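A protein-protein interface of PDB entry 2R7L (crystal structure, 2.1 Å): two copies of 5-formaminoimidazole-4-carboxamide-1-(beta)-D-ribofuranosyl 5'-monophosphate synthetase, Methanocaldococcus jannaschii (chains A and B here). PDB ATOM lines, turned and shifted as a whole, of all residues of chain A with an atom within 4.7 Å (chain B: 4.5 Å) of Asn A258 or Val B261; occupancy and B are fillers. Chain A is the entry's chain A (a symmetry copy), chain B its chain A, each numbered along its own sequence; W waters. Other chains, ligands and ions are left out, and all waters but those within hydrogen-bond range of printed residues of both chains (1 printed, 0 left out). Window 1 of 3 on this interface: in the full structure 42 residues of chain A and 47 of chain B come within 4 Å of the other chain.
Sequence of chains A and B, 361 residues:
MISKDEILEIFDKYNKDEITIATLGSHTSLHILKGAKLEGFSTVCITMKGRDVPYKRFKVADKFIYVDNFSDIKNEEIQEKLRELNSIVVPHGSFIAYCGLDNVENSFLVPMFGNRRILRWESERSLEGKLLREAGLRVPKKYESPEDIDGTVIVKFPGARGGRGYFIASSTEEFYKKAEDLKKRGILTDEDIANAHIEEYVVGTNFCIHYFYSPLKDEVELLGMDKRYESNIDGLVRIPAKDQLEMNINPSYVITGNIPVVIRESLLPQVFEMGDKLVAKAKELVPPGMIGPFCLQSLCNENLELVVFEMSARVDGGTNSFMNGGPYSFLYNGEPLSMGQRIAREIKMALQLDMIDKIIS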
ATOM      1  N   ASP A 226      19.228   0.251 -31.233  1.00  0.00           N
ATOM      2  CA  ASP A 226      17.994  -0.448 -30.883  1.00  0.00           C
ATOM      3  C   ASP A 226      16.799   0.262 -31.512  1.00  0.00           C
ATOM      4  O   ASP A 226      16.895   1.415 -31.949  1.00  0.00           O
ATOM      5  CB  ASP A 226      17.803  -0.503 -29.360  1.00  0.00           C
ATOM      6  CG  ASP A 226      17.477   0.867 -28.757  1.00  0.00           C
ATOM      7  OD1 ASP A 226      18.396   1.710 -28.692  1.00  0.00           O
ATOM      8  OD2 ASP A 226      16.313   1.097 -28.333  1.00  0.00           O
ATOM      9  N   LYS A 227      15.675  -0.438 -31.567  1.00  0.00           N
ATOM     10  CA  LYS A 227      14.406   0.208 -31.859  1.00  0.00           C
ATOM     11  C   LYS A 227      13.534   0.088 -30.619  1.00  0.00           C
ATOM     12  O   LYS A 227      13.592  -0.917 -29.908  1.00  0.00           O
ATOM     13  CB  LYS A 227      13.741  -0.387 -33.105  1.00  0.00           C
ATOM     14  CG  LYS A 227      13.143  -1.760 -32.934  1.00  0.00           C
ATOM     15  CD  LYS A 227      12.201  -2.076 -34.081  1.00  0.00           C
ATOM     16  CE  LYS A 227      11.354  -3.283 -33.765  1.00  0.00           C
ATOM     17  NZ  LYS A 227      10.180  -3.396 -34.659  1.00  0.00           N
ATOM     18  N   ARG A 228      12.751   1.126 -30.347  1.00  0.00           N
ATOM     19  CA  ARG A 228      11.946   1.176 -29.136  1.00  0.00           C
ATOM     20  C   ARG A 228      10.807   0.178 -29.196  1.00  0.00           C
ATOM     21  O   ARG A 228      10.309  -0.145 -30.277  1.00  0.00           O
ATOM     22  CB  ARG A 228      11.358   2.573 -28.933  1.00  0.00           C
ATOM     23  CG  ARG A 228      12.373   3.690 -28.892  1.00  0.00           C
ATOM     24  CD  ARG A 228      13.381   3.456 -27.789  1.00  0.00           C
ATOM     25  NE  ARG A 228      13.872   4.712 -27.237  1.00  0.00           N
ATOM     26  CZ  ARG A 228      15.095   4.890 -26.751  1.00  0.00           C
ATOM     27  NH1 ARG A 228      15.968   3.891 -26.754  1.00  0.00           N
ATOM     28  NH2 ARG A 228      15.446   6.073 -26.266  1.00  0.00           N
ATOM     29  N   TYR A 229      10.398  -0.290 -28.020  1.00  0.00           N
ATOM     30  CA  TYR A 229       9.258  -1.182 -27.865  1.00  0.00           C
ATOM     31  C   TYR A 229       8.363  -0.464 -26.871  1.00  0.00           C
ATOM     32  O   TYR A 229       8.634  -0.452 -25.664  1.00  0.00           O
ATOM     33  CB  TYR A 229       9.720  -2.533 -27.317  1.00  0.00           C
ATOM     34  CG  TYR A 229       8.784  -3.685 -27.560  1.00  0.00           C
ATOM     35  CD1 TYR A 229       8.037  -3.758 -28.721  1.00  0.00           C
ATOM     36  CD2 TYR A 229       8.679  -4.725 -26.648  1.00  0.00           C
ATOM     37  CE1 TYR A 229       7.195  -4.806 -28.959  1.00  0.00           C
ATOM     38  CE2 TYR A 229       7.837  -5.795 -26.885  1.00  0.00           C
ATOM     39  CZ  TYR A 229       7.097  -5.821 -28.043  1.00  0.00           C
ATOM     40  OH  TYR A 229       6.245  -6.861 -28.307  1.00  0.00           O
ATOM     41  N   ILE A 255       7.798   3.980 -23.020  1.00  0.00           N
ATOM     42  CA  ILE A 255       8.914   3.057 -23.253  1.00  0.00           C
ATOM     43  C   ILE A 255       8.829   1.847 -22.335  1.00  0.00           C
ATOM     44  O   ILE A 255       8.764   1.989 -21.109  1.00  0.00           O
ATOM     45  CB  ILE A 255      10.312   3.730 -23.113  1.00  0.00           C
ATOM     46  CG1 ILE A 255      11.398   2.813 -23.676  1.00  0.00           C
ATOM     47  CG2 ILE A 255      10.623   4.081 -21.658  1.00  0.00           C
ATOM     48  CD1 ILE A 255      11.233   2.515 -25.158  1.00  0.00           C
ATOM     49  N   GLY A 257      10.711  -1.276 -23.431  1.00  0.00           N
ATOM     50  CA  GLY A 257      11.783  -2.193 -23.785  1.00  0.00           C
ATOM     51  C   GLY A 257      12.406  -1.872 -25.120  1.00  0.00           C
ATOM     52  O   GLY A 257      12.035  -0.889 -25.764  1.00  0.00           O
ATOM     53  N   ASN A 258      13.358  -2.704 -25.535  1.00  0.00           N
ATOM     54  CA  ASN A 258      14.132  -2.440 -26.734  1.00  0.00           C
ATOM     55  C   ASN A 258      14.401  -3.714 -27.520  1.00  0.00           C
ATOM     56  O   ASN A 258      14.499  -4.800 -26.964  1.00  0.00           O
ATOM     57  CB  ASN A 258      15.461  -1.746 -26.389  1.00  0.00           C
ATOM     58  CG  ASN A 258      15.291  -0.604 -25.394  1.00  0.00           C
ATOM     59  OD1 ASN A 258      15.315   0.572 -25.766  1.00  0.00           O
ATOM     60  ND2 ASN A 258      15.122  -0.947 -24.125  1.00  0.00           N
ATOM     61  N   ILE A 259      14.531  -3.554 -28.827  1.00  0.00           N
ATOM     62  CA  ILE A 259      14.754  -4.657 -29.735  1.00  0.00           C
ATOM     63  C   ILE A 259      16.019  -4.301 -30.511  1.00  0.00           C
ATOM     64  O   ILE A 259      16.197  -3.147 -30.884  1.00  0.00           O
ATOM     65  CB  ILE A 259      13.542  -4.788 -30.668  1.00  0.00           C
ATOM     66  CG1 ILE A 259      12.286  -5.143 -29.849  1.00  0.00           C
ATOM     67  CG2 ILE A 259      13.778  -5.795 -31.775  1.00  0.00           C
ATOM     68  CD1 ILE A 259      10.985  -5.013 -30.629  1.00  0.00           C
ATOM     69  N   PRO A 260      16.928  -5.270 -30.698  1.00  0.00           N
ATOM     70  CA  PRO A 260      18.141  -5.022 -31.478  1.00  0.00           C
ATOM     71  C   PRO A 260      17.845  -4.850 -32.960  1.00  0.00           C
ATOM     72  O   PRO A 260      16.928  -5.470 -33.485  1.00  0.00           O
ATOM     73  CB  PRO A 260      18.982  -6.284 -31.252  1.00  0.00           C
ATOM     74  CG  PRO A 260      18.013  -7.336 -30.806  1.00  0.00           C
ATOM     75  CD  PRO A 260      16.880  -6.635 -30.136  1.00  0.00           C
ATOM     76  N   GLY A 317      18.816   4.502 -22.498  1.00  0.00           N
ATOM     77  CA  GLY A 317      18.313   3.217 -22.008  1.00  0.00           C
ATOM     78  C   GLY A 317      18.410   2.065 -22.993  1.00  0.00           C
ATOM     79  O   GLY A 317      18.444   0.904 -22.592  1.00  0.00           O
ATOM     80  N   GLY A 318      18.442   2.381 -24.283  1.00  0.00           N
ATOM     81  CA  GLY A 318      18.468   1.354 -25.314  1.00  0.00           C
ATOM     82  C   GLY A 318      19.757   0.551 -25.409  1.00  0.00           C
ATOM     83  O   GLY A 318      19.804  -0.469 -26.111  1.00  0.00           O
ATOM     84  N   SER A 321      19.922  -3.264 -24.842  1.00  0.00           N
ATOM     85  CA  SER A 321      19.721  -4.296 -25.854  1.00  0.00           C
ATOM     86  C   SER A 321      21.014  -5.052 -26.199  1.00  0.00           C
ATOM     87  O   SER A 321      20.951  -6.188 -26.671  1.00  0.00           O
ATOM     88  CB  SER A 321      19.081  -3.716 -27.129  1.00  0.00           C
ATOM     89  OG  SER A 321      19.915  -2.725 -27.700  1.00  0.00           O
ATOM     90  N   ASN B 206       4.681  -7.485 -25.736  1.00  0.00           N
ATOM     91  CA  ASN B 206       4.954  -8.858 -25.330  1.00  0.00           C
ATOM     92  C   ASN B 206       6.366  -9.081 -24.775  1.00  0.00           C
ATOM     93  O   ASN B 206       7.373  -8.767 -25.424  1.00  0.00           O
ATOM     94  CB  ASN B 206       4.726  -9.803 -26.505  1.00  0.00           C
ATOM     95  CG  ASN B 206       4.895 -11.267 -26.126  1.00  0.00           C
ATOM     96  OD1 ASN B 206       5.345 -12.065 -26.939  1.00  0.00           O
ATOM     97  ND2 ASN B 206       4.522 -11.626 -24.898  1.00  0.00           N
ATOM     98  N   PHE B 207       6.418  -9.625 -23.568  1.00  0.00           N
ATOM     99  CA  PHE B 207       7.661 -10.077 -22.956  1.00  0.00           C
ATOM    100  C   PHE B 207       7.414 -11.475 -22.434  1.00  0.00           C
ATOM    101  O   PHE B 207       6.697 -11.646 -21.455  1.00  0.00           O
ATOM    102  CB  PHE B 207       8.029  -9.181 -21.774  1.00  0.00           C
ATOM    103  CG  PHE B 207       8.367  -7.772 -22.163  1.00  0.00           C
ATOM    104  CD1 PHE B 207       9.654  -7.436 -22.548  1.00  0.00           C
ATOM    105  CD2 PHE B 207       7.397  -6.776 -22.128  1.00  0.00           C
ATOM    106  CE1 PHE B 207       9.974  -6.131 -22.899  1.00  0.00           C
ATOM    107  CE2 PHE B 207       7.707  -5.477 -22.480  1.00  0.00           C
ATOM    108  CZ  PHE B 207       9.007  -5.156 -22.874  1.00  0.00           C
ATOM    109  N   MET B 225      14.557 -13.069 -22.406  1.00  0.00           N
ATOM    110  CA  MET B 225      13.207 -12.684 -22.819  1.00  0.00           C
ATOM    111  C   MET B 225      13.119 -12.664 -24.329  1.00  0.00           C
ATOM    112  O   MET B 225      14.089 -12.304 -25.012  1.00  0.00           O
ATOM    113  CB  MET B 225      12.869 -11.268 -22.325  1.00  0.00           C
ATOM    114  CG  MET B 225      13.003 -11.038 -20.835  1.00  0.00           C
ATOM    115  SD  MET B 225      12.548  -9.331 -20.451  1.00  0.00           S
ATOM    116  CE  MET B 225      12.812  -9.291 -18.678  1.00  0.00           C
ATOM    117  N   ASP B 226      11.945 -13.014 -24.843  1.00  0.00           N
ATOM    118  CA  ASP B 226      11.649 -12.887 -26.268  1.00  0.00           C
ATOM    119  C   ASP B 226      10.244 -12.325 -26.458  1.00  0.00           C
ATOM    120  O   ASP B 226       9.425 -12.318 -25.531  1.00  0.00           O
ATOM    121  CB  ASP B 226      11.748 -14.247 -26.975  1.00  0.00           C
ATOM    122  CG  ASP B 226      10.614 -15.200 -26.582  1.00  0.00           C
ATOM    123  OD1 ASP B 226      10.643 -15.702 -25.439  1.00  0.00           O
ATOM    124  OD2 ASP B 226       9.706 -15.461 -27.416  1.00  0.00           O
ATOM    125  N   LYS B 227       9.972 -11.843 -27.663  1.00  0.00           N
ATOM    126  CA  LYS B 227       8.605 -11.559 -28.063  1.00  0.00           C
ATOM    127  C   LYS B 227       8.250 -12.513 -29.192  1.00  0.00           C
ATOM    128  O   LYS B 227       9.100 -12.852 -30.017  1.00  0.00           O
ATOM    129  CB  LYS B 227       8.423 -10.090 -28.457  1.00  0.00           C
ATOM    130  CG  LYS B 227       9.024  -9.689 -29.780  1.00  0.00           C
ATOM    131  CD  LYS B 227       8.466  -8.353 -30.234  1.00  0.00           C
ATOM    132  CE  LYS B 227       8.795  -8.097 -31.684  1.00  0.00           C
ATOM    133  NZ  LYS B 227       7.963  -7.020 -32.268  1.00  0.00           N
ATOM    134  N   ILE B 259      11.774 -13.153 -31.345  1.00  0.00           N
ATOM    135  CA  ILE B 259      12.608 -11.986 -31.541  1.00  0.00           C
ATOM    136  C   ILE B 259      13.119 -11.611 -30.153  1.00  0.00           C
ATOM    137  O   ILE B 259      12.364 -11.677 -29.189  1.00  0.00           O
ATOM    138  CB  ILE B 259      11.758 -10.862 -32.149  1.00  0.00           C
ATOM    139  CG1 ILE B 259      11.257 -11.280 -33.546  1.00  0.00           C
ATOM    140  CG2 ILE B 259      12.507  -9.546 -32.206  1.00  0.00           C
ATOM    141  CD1 ILE B 259      10.177 -10.368 -34.111  1.00  0.00           C
ATOM    142  N   PRO B 260      14.414 -11.280 -30.035  1.00  0.00           N
ATOM    143  CA  PRO B 260      14.968 -10.855 -28.749  1.00  0.00           C
ATOM    144  C   PRO B 260      14.457  -9.484 -28.329  1.00  0.00           C
ATOM    145  O   PRO B 260      14.211  -8.630 -29.172  1.00  0.00           O
ATOM    146  CB  PRO B 260      16.477 -10.798 -29.004  1.00  0.00           C
ATOM    147  CG  PRO B 260      16.629 -10.692 -30.491  1.00  0.00           C
ATOM    148  CD  PRO B 260      15.433 -11.343 -31.102  1.00  0.00           C
ATOM    149  N   VAL B 261      14.313  -9.287 -27.022  1.00  0.00           N
ATOM    150  CA  VAL B 261      13.868  -8.024 -26.472  1.00  0.00           C
ATOM    151  C   VAL B 261      14.430  -7.917 -25.061  1.00  0.00           C
ATOM    152  O   VAL B 261      14.724  -8.928 -24.430  1.00  0.00           O
ATOM    153  CB  VAL B 261      12.307  -7.950 -26.432  1.00  0.00           C
ATOM    154  CG1 VAL B 261      11.735  -8.937 -25.404  1.00  0.00           C
ATOM    155  CG2 VAL B 261      11.842  -6.534 -26.129  1.00  0.00           C
ATOM    156  N   VAL B 262      14.617  -6.693 -24.584  1.00  0.00           N
ATOM    157  CA  VAL B 262      14.973  -6.462 -23.200  1.00  0.00           C
ATOM    158  C   VAL B 262      13.928  -5.525 -22.640  1.00  0.00           C
ATOM    159  O   VAL B 262      13.315  -4.770 -23.378  1.00  0.00           O
ATOM    160  CB  VAL B 262      16.394  -5.819 -23.028  1.00  0.00           C
ATOM    161  CG1 VAL B 262      17.499  -6.788 -23.456  1.00  0.00           C
ATOM    162  CG2 VAL B 262      16.497  -4.504 -23.781  1.00  0.00           C
ATOM    163  N   ILE B 263      13.723  -5.575 -21.334  1.00  0.00           N
ATOM    164  CA  ILE B 263      12.718  -4.744 -20.702  1.00  0.00           C
ATOM    165  C   ILE B 263      13.362  -3.491 -20.116  1.00  0.00           C
ATOM    166  O   ILE B 263      14.570  -3.455 -19.877  1.00  0.00           O
ATOM    167  CB  ILE B 263      11.982  -5.520 -19.591  1.00  0.00           C
ATOM    168  CG1 ILE B 263      10.574  -4.953 -19.363  1.00  0.00           C
ATOM    169  CG2 ILE B 263      12.798  -5.507 -18.298  1.00  0.00           C
ATOM    170  CD1 ILE B 263       9.683  -5.855 -18.508  1.00  0.00           C
HETATM  171  O   HOH W   1      15.765  -1.815 -21.457  1.00  0.00           O
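OH of Tyr A229 is in hydrogen-bond range of N of Asn B206 (3.1 Å).
O of Val B262 lies within hydrogen-bond range of N of Asn A258 (3.0 Å).
O of Ile B259 sits at hydrogen-bond distance from N of Lys B227 (2.8 Å).
The side-chain amide oxygen (OD1) of Asn A258 lies close to the side-chain carboxylate (OD2) of Asp A226 (2.8 Å).
The backbone NH (N) of Lys A227 is in hydrogen-bond range of the backbone carbonyl oxygen (O) of Ile A259 (2.8 Å).
N of Tyr A229 sits at hydrogen-bond distance from O of Gly A257.
OG of Ser A321 lies within hydrogen-bond range of O of Gly A318, at 2.8 Å.
CD of Lys B227 touches OH of Tyr A229 (3.3 Å).
Val B261 touches Tyr A229.
CA of Gly A257 touches O of Val B262, at 3.0 Å.
CG2 of Val B261 touches O of Asn A258, 3.3 Å away.
Ile A259 touches Lys B227 (CD1 to CE, 3.9 Å).
Ile A259 touches Ile B259 (CG2 to CG2, 3.98 Å).
Pro B260 touches Ile A259 (O to CG2, 3.9 Å).
Ile A259 touches Val B261 (CG1 to CG2, 3.996 Å).
Pro A260 touches Pro B260.
Ser A321 touches Val B262.
Ile A255 touches none of the printed residues of chain B.
Of chain B, only Val B261 (3.3 Å) and Val B262 (3.0 Å) come within 4 Å of Asn A258.
Of the printed residues of chain A, Asn B206 touches Tyr A229 (3.1 Å).
Of the printed residues of chain A, Pro B260 touches Ile A259 (3.9 Å) and Pro A260 (3.5 Å).
Printed residues of chain A within 4 Å of Val B261: Tyr A229, Asn A258 and Ile A259.
Of the printed residues of chain A, Val B262 touches Gly A257, Asn A258 and Ser A321.
The nearest residue of chain B that does not touch Asn A258 is Pro B260 (4.4 Å).
The nearest printed residue of chain A that does not touch Val B261 is Gly A257 (4.8 Å).
The nearest printed residue of chain A that does not touch Lys B227 is Lys A227 (4.9 Å).
Hydrophobic or aromatic side chains of chain A within 4 Å of the printed part of chain B: Tyr A229, Ile A259 and Pro A260.
Among the printed residues, no Asp or Glu carboxylate lies within 4 Å of a Lys or Arg side-chain nitrogen of the other chain.
Ile A259 touches Lys B227, but with the chains exchanged Lys A227 does not touch Ile B259 (6.6 Å).
Ile B259 touches its own counterpart, Ile A259.
Ile A259 touches Pro B260, but with the chains exchanged Pro A260 does not touch Ile B259 (5.6 Å).
Pro A260 touches its own counterpart, Pro B260.
Of the 13 pairs that touch across the chains among the printed residues, 2 have their exchanged pair printed and touching as well.
Water W1 bridges the backbone carbonyl oxygen (O) of Ile B263 (2.6 Å) and the side-chain amide nitrogen (ND2) of Asn A258 (2.9 Å).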
